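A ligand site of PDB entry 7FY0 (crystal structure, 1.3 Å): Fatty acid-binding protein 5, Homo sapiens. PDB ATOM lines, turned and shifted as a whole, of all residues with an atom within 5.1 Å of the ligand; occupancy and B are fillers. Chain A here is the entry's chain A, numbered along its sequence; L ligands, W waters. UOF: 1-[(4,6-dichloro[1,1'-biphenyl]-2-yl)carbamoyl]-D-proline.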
ATOM      1  N   PHE A  22     -25.876  23.981  30.197  1.00  0.00           N
ATOM      2  CA  PHE A  22     -25.107  23.922  28.953  1.00  0.00           C
ATOM      3  C   PHE A  22     -23.629  23.560  29.214  1.00  0.00           C
ATOM      4  O   PHE A  22     -23.049  22.734  28.492  1.00  0.00           O
ATOM      5  CB  PHE A  22     -25.193  25.253  28.211  1.00  0.00           C
ATOM      6  CG  PHE A  22     -24.590  25.205  26.860  1.00  0.00           C
ATOM      7  CD1 PHE A  22     -24.904  24.219  25.962  1.00  0.00           C
ATOM      8  CD2 PHE A  22     -23.712  26.209  26.485  1.00  0.00           C
ATOM      9  CE1 PHE A  22     -24.347  24.205  24.711  1.00  0.00           C
ATOM     10  CE2 PHE A  22     -23.143  26.197  25.212  1.00  0.00           C
ATOM     11  CZ  PHE A  22     -23.473  25.200  24.346  1.00  0.00           C
ATOM     12  N   TYR A  25     -23.560  19.858  29.803  1.00  0.00           N
ATOM     13  CA  TYR A  25     -23.674  19.150  28.518  1.00  0.00           C
ATOM     14  C   TYR A  25     -22.347  19.137  27.765  1.00  0.00           C
ATOM     15  O   TYR A  25     -21.926  18.114  27.236  1.00  0.00           O
ATOM     16  CB  TYR A  25     -24.807  19.771  27.706  1.00  0.00           C
ATOM     17  CG  TYR A  25     -24.955  19.270  26.298  1.00  0.00           C
ATOM     18  CD1 TYR A  25     -25.508  18.013  26.050  1.00  0.00           C
ATOM     19  CD2 TYR A  25     -24.576  20.027  25.221  1.00  0.00           C
ATOM     20  CE1 TYR A  25     -25.676  17.541  24.769  1.00  0.00           C
ATOM     21  CE2 TYR A  25     -24.733  19.543  23.935  1.00  0.00           C
ATOM     22  CZ  TYR A  25     -25.256  18.288  23.704  1.00  0.00           C
ATOM     23  OH  TYR A  25     -25.446  17.821  22.426  1.00  0.00           O
ATOM     24  N   MET A  26     -21.671  20.283  27.728  1.00  0.00           N
ATOM     25  CA  MET A  26     -20.331  20.353  27.093  1.00  0.00           C
ATOM     26  C   MET A  26     -19.313  19.444  27.772  1.00  0.00           C
ATOM     27  O   MET A  26     -18.523  18.814  27.100  1.00  0.00           O
ATOM     28  CB  MET A  26     -19.805  21.780  27.058  1.00  0.00           C
ATOM     29  CG  MET A  26     -20.565  22.666  26.073  1.00  0.00           C
ATOM     30  SD  MET A  26     -19.814  24.299  25.797  1.00  0.00           S
ATOM     31  CE  MET A  26     -20.196  25.065  27.368  1.00  0.00           C
ATOM     32  N   LEU A  29     -19.850  15.862  26.718  1.00  0.00           N
ATOM     33  CA  LEU A  29     -19.258  15.677  25.398  1.00  0.00           C
ATOM     34  C   LEU A  29     -17.714  15.607  25.485  1.00  0.00           C
ATOM     35  O   LEU A  29     -17.083  15.115  24.549  1.00  0.00           O
ATOM     36  CB  LEU A  29     -19.637  16.807  24.458  1.00  0.00           C
ATOM     37  CG  LEU A  29     -20.996  16.661  23.816  1.00  0.00           C
ATOM     38  CD1 LEU A  29     -21.432  18.041  23.336  1.00  0.00           C
ATOM     39  CD2 LEU A  29     -21.011  15.603  22.729  1.00  0.00           C
ATOM     40  N   VAL A  31     -15.846  18.400  25.737  1.00  0.00           N
ATOM     41  CA  VAL A  31     -15.375  19.627  25.073  1.00  0.00           C
ATOM     42  C   VAL A  31     -14.332  20.245  26.005  1.00  0.00           C
ATOM     43  O   VAL A  31     -14.506  20.278  27.244  1.00  0.00           O
ATOM     44  CB  VAL A  31     -16.544  20.639  24.802  1.00  0.00           C
ATOM     45  CG1 VAL A  31     -16.025  21.955  24.192  1.00  0.00           C
ATOM     46  CG2 VAL A  31     -17.577  19.993  23.882  1.00  0.00           C
ATOM     47  N   LEU A  35     -13.062  25.956  24.547  1.00  0.00           N
ATOM     48  CA  LEU A  35     -14.381  25.978  23.920  1.00  0.00           C
ATOM     49  C   LEU A  35     -15.505  26.092  24.980  1.00  0.00           C
ATOM     50  O   LEU A  35     -16.476  26.786  24.748  1.00  0.00           O
ATOM     51  CB  LEU A  35     -14.584  24.763  23.022  1.00  0.00           C
ATOM     52  CG  LEU A  35     -13.877  24.707  21.675  1.00  0.00           C
ATOM     53  CD1 LEU A  35     -13.907  23.296  21.101  1.00  0.00           C
ATOM     54  CD2 LEU A  35     -14.482  25.712  20.675  1.00  0.00           C
ATOM     55  N   MET A  38     -15.862  29.680  25.996  1.00  0.00           N
ATOM     56  CA  MET A  38     -16.544  30.400  24.939  1.00  0.00           C
ATOM     57  C   MET A  38     -18.074  30.146  25.019  1.00  0.00           C
ATOM     58  O   MET A  38     -18.873  31.078  24.909  1.00  0.00           O
ATOM     59  CB  MET A  38     -15.968  30.021  23.578  1.00  0.00           C
ATOM     60  CG  MET A  38     -14.503  30.349  23.410  1.00  0.00           C
ATOM     61  SD  MET A  38     -14.128  32.090  23.659  1.00  0.00           S
ATOM     62  CE  MET A  38     -12.897  32.373  22.402  1.00  0.00           C
ATOM     63  N   GLY A  39     -18.467  28.886  25.237  1.00  0.00           N
ATOM     64  CA  GLY A  39     -19.895  28.530  25.334  1.00  0.00           C
ATOM     65  C   GLY A  39     -20.618  29.030  26.566  1.00  0.00           C
ATOM     66  O   GLY A  39     -21.830  29.339  26.516  1.00  0.00           O
ATOM     67  N   ALA A  42     -20.734  33.136  25.628  1.00  0.00           N
ATOM     68  CA  ALA A  42     -21.397  33.600  24.403  1.00  0.00           C
ATOM     69  C   ALA A  42     -22.939  33.733  24.565  1.00  0.00           C
ATOM     70  O   ALA A  42     -23.581  32.983  25.313  1.00  0.00           O
ATOM     71  CB  ALA A  42     -21.040  32.704  23.226  1.00  0.00           C
ATOM     72  N   PRO A  44     -25.304  33.748  21.702  1.00  0.00           N
ATOM     73  CA  PRO A  44     -25.562  33.676  20.257  1.00  0.00           C
ATOM     74  C   PRO A  44     -26.975  34.009  19.824  1.00  0.00           C
ATOM     75  O   PRO A  44     -27.974  33.926  20.601  1.00  0.00           O
ATOM     76  CB  PRO A  44     -25.238  32.244  19.920  1.00  0.00           C
ATOM     77  CG  PRO A  44     -25.557  31.488  21.188  1.00  0.00           C
ATOM     78  CD  PRO A  44     -25.172  32.405  22.304  1.00  0.00           C
ATOM     79  N   SER A  61     -22.257  34.824  16.809  1.00  0.00           N
ATOM     80  CA  SER A  61     -21.766  35.545  17.996  1.00  0.00           C
ATOM     81  C   SER A  61     -20.344  35.942  17.737  1.00  0.00           C
ATOM     82  O   SER A  61     -19.755  35.402  16.791  1.00  0.00           O
ATOM     83  CB  SER A  61     -21.883  34.706  19.287  1.00  0.00           C
ATOM     84  OG  SER A  61     -21.002  33.588  19.284  1.00  0.00           O
ATOM     85  N   THR A  80     -19.972  19.847  13.792  1.00  0.00           N
ATOM     86  CA  THR A  80     -20.454  20.571  14.940  1.00  0.00           C
ATOM     87  C   THR A  80     -19.434  21.652  15.359  1.00  0.00           C
ATOM     88  O   THR A  80     -18.276  21.593  14.957  1.00  0.00           O
ATOM     89  CB  THR A  80     -20.761  19.613  16.106  1.00  0.00           C
ATOM     90  OG1 THR A  80     -19.558  19.060  16.623  1.00  0.00           O
ATOM     91  CG2 THR A  80     -21.773  18.491  15.669  1.00  0.00           C
ATOM     92  N   ALA A  81     -19.826  22.596  16.222  1.00  0.00           N
ATOM     93  CA  ALA A  81     -18.888  23.674  16.657  1.00  0.00           C
ATOM     94  C   ALA A  81     -17.643  23.149  17.358  1.00  0.00           C
ATOM     95  O   ALA A  81     -16.550  23.713  17.253  1.00  0.00           O
ATOM     96  CB  ALA A  81     -19.596  24.721  17.545  1.00  0.00           C
ATOM     97  N   ASP A  82     -17.849  22.121  18.186  1.00  0.00           N
ATOM     98  CA  ASP A  82     -16.766  21.455  18.882  1.00  0.00           C
ATOM     99  C   ASP A  82     -15.946  20.536  17.984  1.00  0.00           C
ATOM    100  O   ASP A  82     -14.981  19.969  18.444  1.00  0.00           O
ATOM    101  CB  ASP A  82     -17.269  20.734  20.128  1.00  0.00           C
ATOM    102  CG  ASP A  82     -18.308  19.640  19.805  1.00  0.00           C
ATOM    103  OD1 ASP A  82     -19.302  19.931  19.139  1.00  0.00           O
ATOM    104  OD2 ASP A  82     -18.096  18.496  20.285  1.00  0.00           O
ATOM    105  N   ARG A  84     -16.896  17.717  15.976  1.00  0.00           N
ATOM    106  CA  ARG A  84     -17.336  16.392  15.597  1.00  0.00           C
ATOM    107  C   ARG A  84     -17.876  16.414  14.176  1.00  0.00           C
ATOM    108  O   ARG A  84     -18.421  17.430  13.736  1.00  0.00           O
ATOM    109  CB  ARG A  84     -18.426  15.900  16.579  1.00  0.00           C
ATOM    110  CG  ARG A  84     -17.934  15.630  18.015  1.00  0.00           C
ATOM    111  CD  ARG A  84     -19.090  15.345  18.944  1.00  0.00           C
ATOM    112  NE  ARG A  84     -19.805  16.595  19.232  1.00  0.00           N
ATOM    113  CZ  ARG A  84     -21.117  16.785  19.194  1.00  0.00           C
ATOM    114  NH1 ARG A  84     -21.990  15.787  18.985  1.00  0.00           N
ATOM    115  NH2 ARG A  84     -21.588  18.012  19.380  1.00  0.00           N
ATOM    116  N   ILE A 110     -30.925  17.101  20.141  1.00  0.00           N
ATOM    117  CA  ILE A 110     -31.302  18.480  20.356  1.00  0.00           C
ATOM    118  C   ILE A 110     -32.737  18.669  19.859  1.00  0.00           C
ATOM    119  O   ILE A 110     -33.032  18.356  18.706  1.00  0.00           O
ATOM    120  CB  ILE A 110     -30.346  19.490  19.613  1.00  0.00           C
ATOM    121  CG1 ILE A 110     -28.874  19.315  20.053  1.00  0.00           C
ATOM    122  CG2 ILE A 110     -30.836  20.926  19.866  1.00  0.00           C
ATOM    123  CD1 ILE A 110     -27.925  19.995  19.110  1.00  0.00           C
ATOM    124  N   ARG A 112     -36.066  21.525  19.428  1.00  0.00           N
ATOM    125  CA  ARG A 112     -36.385  22.949  19.362  1.00  0.00           C
ATOM    126  C   ARG A 112     -37.913  23.067  19.203  1.00  0.00           C
ATOM    127  O   ARG A 112     -38.513  22.429  18.324  1.00  0.00           O
ATOM    128  CB  ARG A 112     -35.700  23.633  18.201  1.00  0.00           C
ATOM    129  CG  ARG A 112     -34.190  23.539  18.235  1.00  0.00           C
ATOM    130  CD  ARG A 112     -33.511  24.348  17.121  1.00  0.00           C
ATOM    131  NE  ARG A 112     -32.050  24.354  17.199  1.00  0.00           N
ATOM    132  CZ  ARG A 112     -31.277  23.342  16.798  1.00  0.00           C
ATOM    133  NH1 ARG A 112     -31.804  22.207  16.408  1.00  0.00           N
ATOM    134  NH2 ARG A 112     -29.941  23.476  16.838  1.00  0.00           N
ATOM    135  N   VAL A 121     -34.858  25.405  23.364  1.00  0.00           N
ATOM    136  CA  VAL A 121     -33.890  24.472  22.811  1.00  0.00           C
ATOM    137  C   VAL A 121     -33.406  23.569  23.938  1.00  0.00           C
ATOM    138  O   VAL A 121     -32.937  24.043  24.963  1.00  0.00           O
ATOM    139  CB  VAL A 121     -32.695  25.223  22.164  1.00  0.00           C
ATOM    140  CG1 VAL A 121     -31.681  24.240  21.574  1.00  0.00           C
ATOM    141  CG2 VAL A 121     -33.207  26.185  21.088  1.00  0.00           C
ATOM    142  N   CYS A 123     -31.158  20.049  24.974  1.00  0.00           N
ATOM    143  CA  CYS A 123     -30.128  19.098  24.541  1.00  0.00           C
ATOM    144  C   CYS A 123     -29.980  17.973  25.538  1.00  0.00           C
ATOM    145  O   CYS A 123     -30.234  18.167  26.748  1.00  0.00           O
ATOM    146  CB  CYS A 123     -28.773  19.775  24.361  1.00  0.00           C
ATOM    147  SG  CYS A 123     -28.808  21.175  23.239  1.00  0.00           S
ATOM    148  N   ARG A 132     -32.213  25.903  26.879  1.00  0.00           N
ATOM    149  CA  ARG A 132     -31.842  27.230  26.474  1.00  0.00           C
ATOM    150  C   ARG A 132     -33.058  27.899  25.849  1.00  0.00           C
ATOM    151  O   ARG A 132     -33.746  27.321  25.012  1.00  0.00           O
ATOM    152  CB  ARG A 132     -30.672  27.218  25.514  1.00  0.00           C
ATOM    153  CG  ARG A 132     -29.404  26.879  26.292  1.00  0.00           C
ATOM    154  CD  ARG A 132     -28.269  26.323  25.498  1.00  0.00           C
ATOM    155  NE  ARG A 132     -27.615  27.236  24.614  1.00  0.00           N
ATOM    156  CZ  ARG A 132     -26.654  28.093  24.919  1.00  0.00           C
ATOM    157  NH1 ARG A 132     -26.292  28.340  26.167  1.00  0.00           N
ATOM    158  NH2 ARG A 132     -26.025  28.721  23.928  1.00  0.00           N
ATOM    159  N   TYR A 134     -34.748  31.253  23.910  1.00  0.00           N
ATOM    160  CA  TYR A 134     -34.493  32.374  23.025  1.00  0.00           C
ATOM    161  C   TYR A 134     -35.744  33.212  22.790  1.00  0.00           C
ATOM    162  O   TYR A 134     -36.851  32.678  22.760  1.00  0.00           O
ATOM    163  CB  TYR A 134     -33.994  31.858  21.674  1.00  0.00           C
ATOM    164  CG  TYR A 134     -32.675  31.108  21.637  1.00  0.00           C
ATOM    165  CD1 TYR A 134     -32.554  29.817  22.141  1.00  0.00           C
ATOM    166  CD2 TYR A 134     -31.573  31.682  21.048  1.00  0.00           C
ATOM    167  CE1 TYR A 134     -31.343  29.127  22.061  1.00  0.00           C
ATOM    168  CE2 TYR A 134     -30.365  31.012  20.992  1.00  0.00           C
ATOM    169  CZ  TYR A 134     -30.236  29.736  21.492  1.00  0.00           C
ATOM    170  OH  TYR A 134     -29.017  29.076  21.391  1.00  0.00           O
HETATM  171  C1  UOF L   1     -22.367  25.970  21.203  1.00  0.00           C
HETATM  172  C2  UOF L   1     -22.202  27.365  21.430  1.00  0.00           C
HETATM  173  C3  UOF L   1     -20.921  27.869  21.738  1.00  0.00           C
HETATM  174  C4  UOF L   1     -19.791  27.014  21.836  1.00  0.00           C
HETATM  175  C5  UOF L   1     -19.931  25.636  21.596  1.00  0.00           C
HETATM  176  C6  UOF L   1     -21.226  25.095  21.272  1.00  0.00           C
HETATM  177 CL7  UOF L   1     -18.512  24.657  21.745  1.00  0.00          CL
HETATM  178 CL8  UOF L   1     -20.735  29.571  22.049  1.00  0.00          CL
HETATM  179  C9  UOF L   1     -21.461  23.659  21.143  1.00  0.00           C
HETATM  180  C10 UOF L   1     -21.314  22.955  22.348  1.00  0.00           C
HETATM  181  C11 UOF L   1     -21.494  21.590  22.442  1.00  0.00           C
HETATM  182  C12 UOF L   1     -21.866  20.910  21.305  1.00  0.00           C
HETATM  183  C13 UOF L   1     -22.010  21.586  20.099  1.00  0.00           C
HETATM  184  C14 UOF L   1     -21.821  22.959  20.024  1.00  0.00           C
HETATM  185  N15 UOF L   1     -23.620  25.363  20.876  1.00  0.00           N
HETATM  186  C16 UOF L   1     -24.896  25.670  21.336  1.00  0.00           C
HETATM  187  N17 UOF L   1     -25.836  24.621  21.341  1.00  0.00           N
HETATM  188  O18 UOF L   1     -25.253  26.803  21.752  1.00  0.00           O
HETATM  189  C19 UOF L   1     -25.646  23.216  20.990  1.00  0.00           C
HETATM  190  C20 UOF L   1     -26.652  22.523  21.858  1.00  0.00           C
HETATM  191  C21 UOF L   1     -27.747  23.466  22.063  1.00  0.00           C
HETATM  192  C22 UOF L   1     -27.125  24.849  21.983  1.00  0.00           C
HETATM  193  C23 UOF L   1     -27.958  25.854  21.227  1.00  0.00           C
HETATM  194  O24 UOF L   1     -28.658  26.661  22.086  1.00  0.00           O
HETATM  195  O25 UOF L   1     -28.043  26.053  20.005  1.00  0.00           O
HETATM  196  O   HOH W   1     -26.421  25.212  17.946  1.00  0.00           O
HETATM  197  O   HOH W   2     -30.554  26.456  18.514  1.00  0.00           O
HETATM  198  O   HOH W   3     -24.850  28.555  19.536  1.00  0.00           O
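An oxygen (O24) of the ligand sits at hydrogen-bond distance from the side-chain hydroxyl of Tyr 134. An oxygen (O24) of the ligand is in salt-bridge range of the guanidinium group of Arg 132 (2.8 Å).
The backbone NH (N) of Val 31 sits at hydrogen-bond distance from the backbone carbonyl oxygen (O) of Met 26 (3.0 Å). The side-chain carboxylate (OD2) of Asp 82 is in salt-bridge range of the guanidinium group (NE) of Arg 84, 2.8 Å away. The backbone carbonyl oxygen (O) of Arg 132 is in hydrogen-bond range of the backbone NH (N) of Val 121. The backbone NH of Arg 84 sits at hydrogen-bond distance from the side-chain hydroxyl of Thr 80 (3.1 Å). OD1 of Asp 82 lies within hydrogen-bond range of OG1 of Thr 80, 2.7 Å away.
Residues that only touch the ligand: Cys 123 (2.8 Å), Asp 82 (3.3 Å), Ala 42 (3.4 Å), Phe 22 (3.4 Å), Arg 84 (3.5 Å), Leu 29 (3.5 Å), Gly 39 (3.5 Å), Met 38 (3.7 Å), Ala 81 (3.8 Å), Met 26 (3.8 Å), Val 121 (3.9 Å) and Ile 110 (3.9 Å). Within 4 Å of the ligand: Phe 22, Met 26, Leu 29, Met 38, Gly 39, Ala 42, Ala 81, Asp 82, Arg 84, Ile 110, Val 121, Cys 123, Arg 132 and Tyr 134. The nearest printed residue that does not touch the ligand is Tyr 25 (4.1 Å).
Water W2 lies within hydrogen-bond range of the guanidinium group (NE) of Arg 112 (2.9 Å) and an oxygen (O25) of the ligand (2.9 Å).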
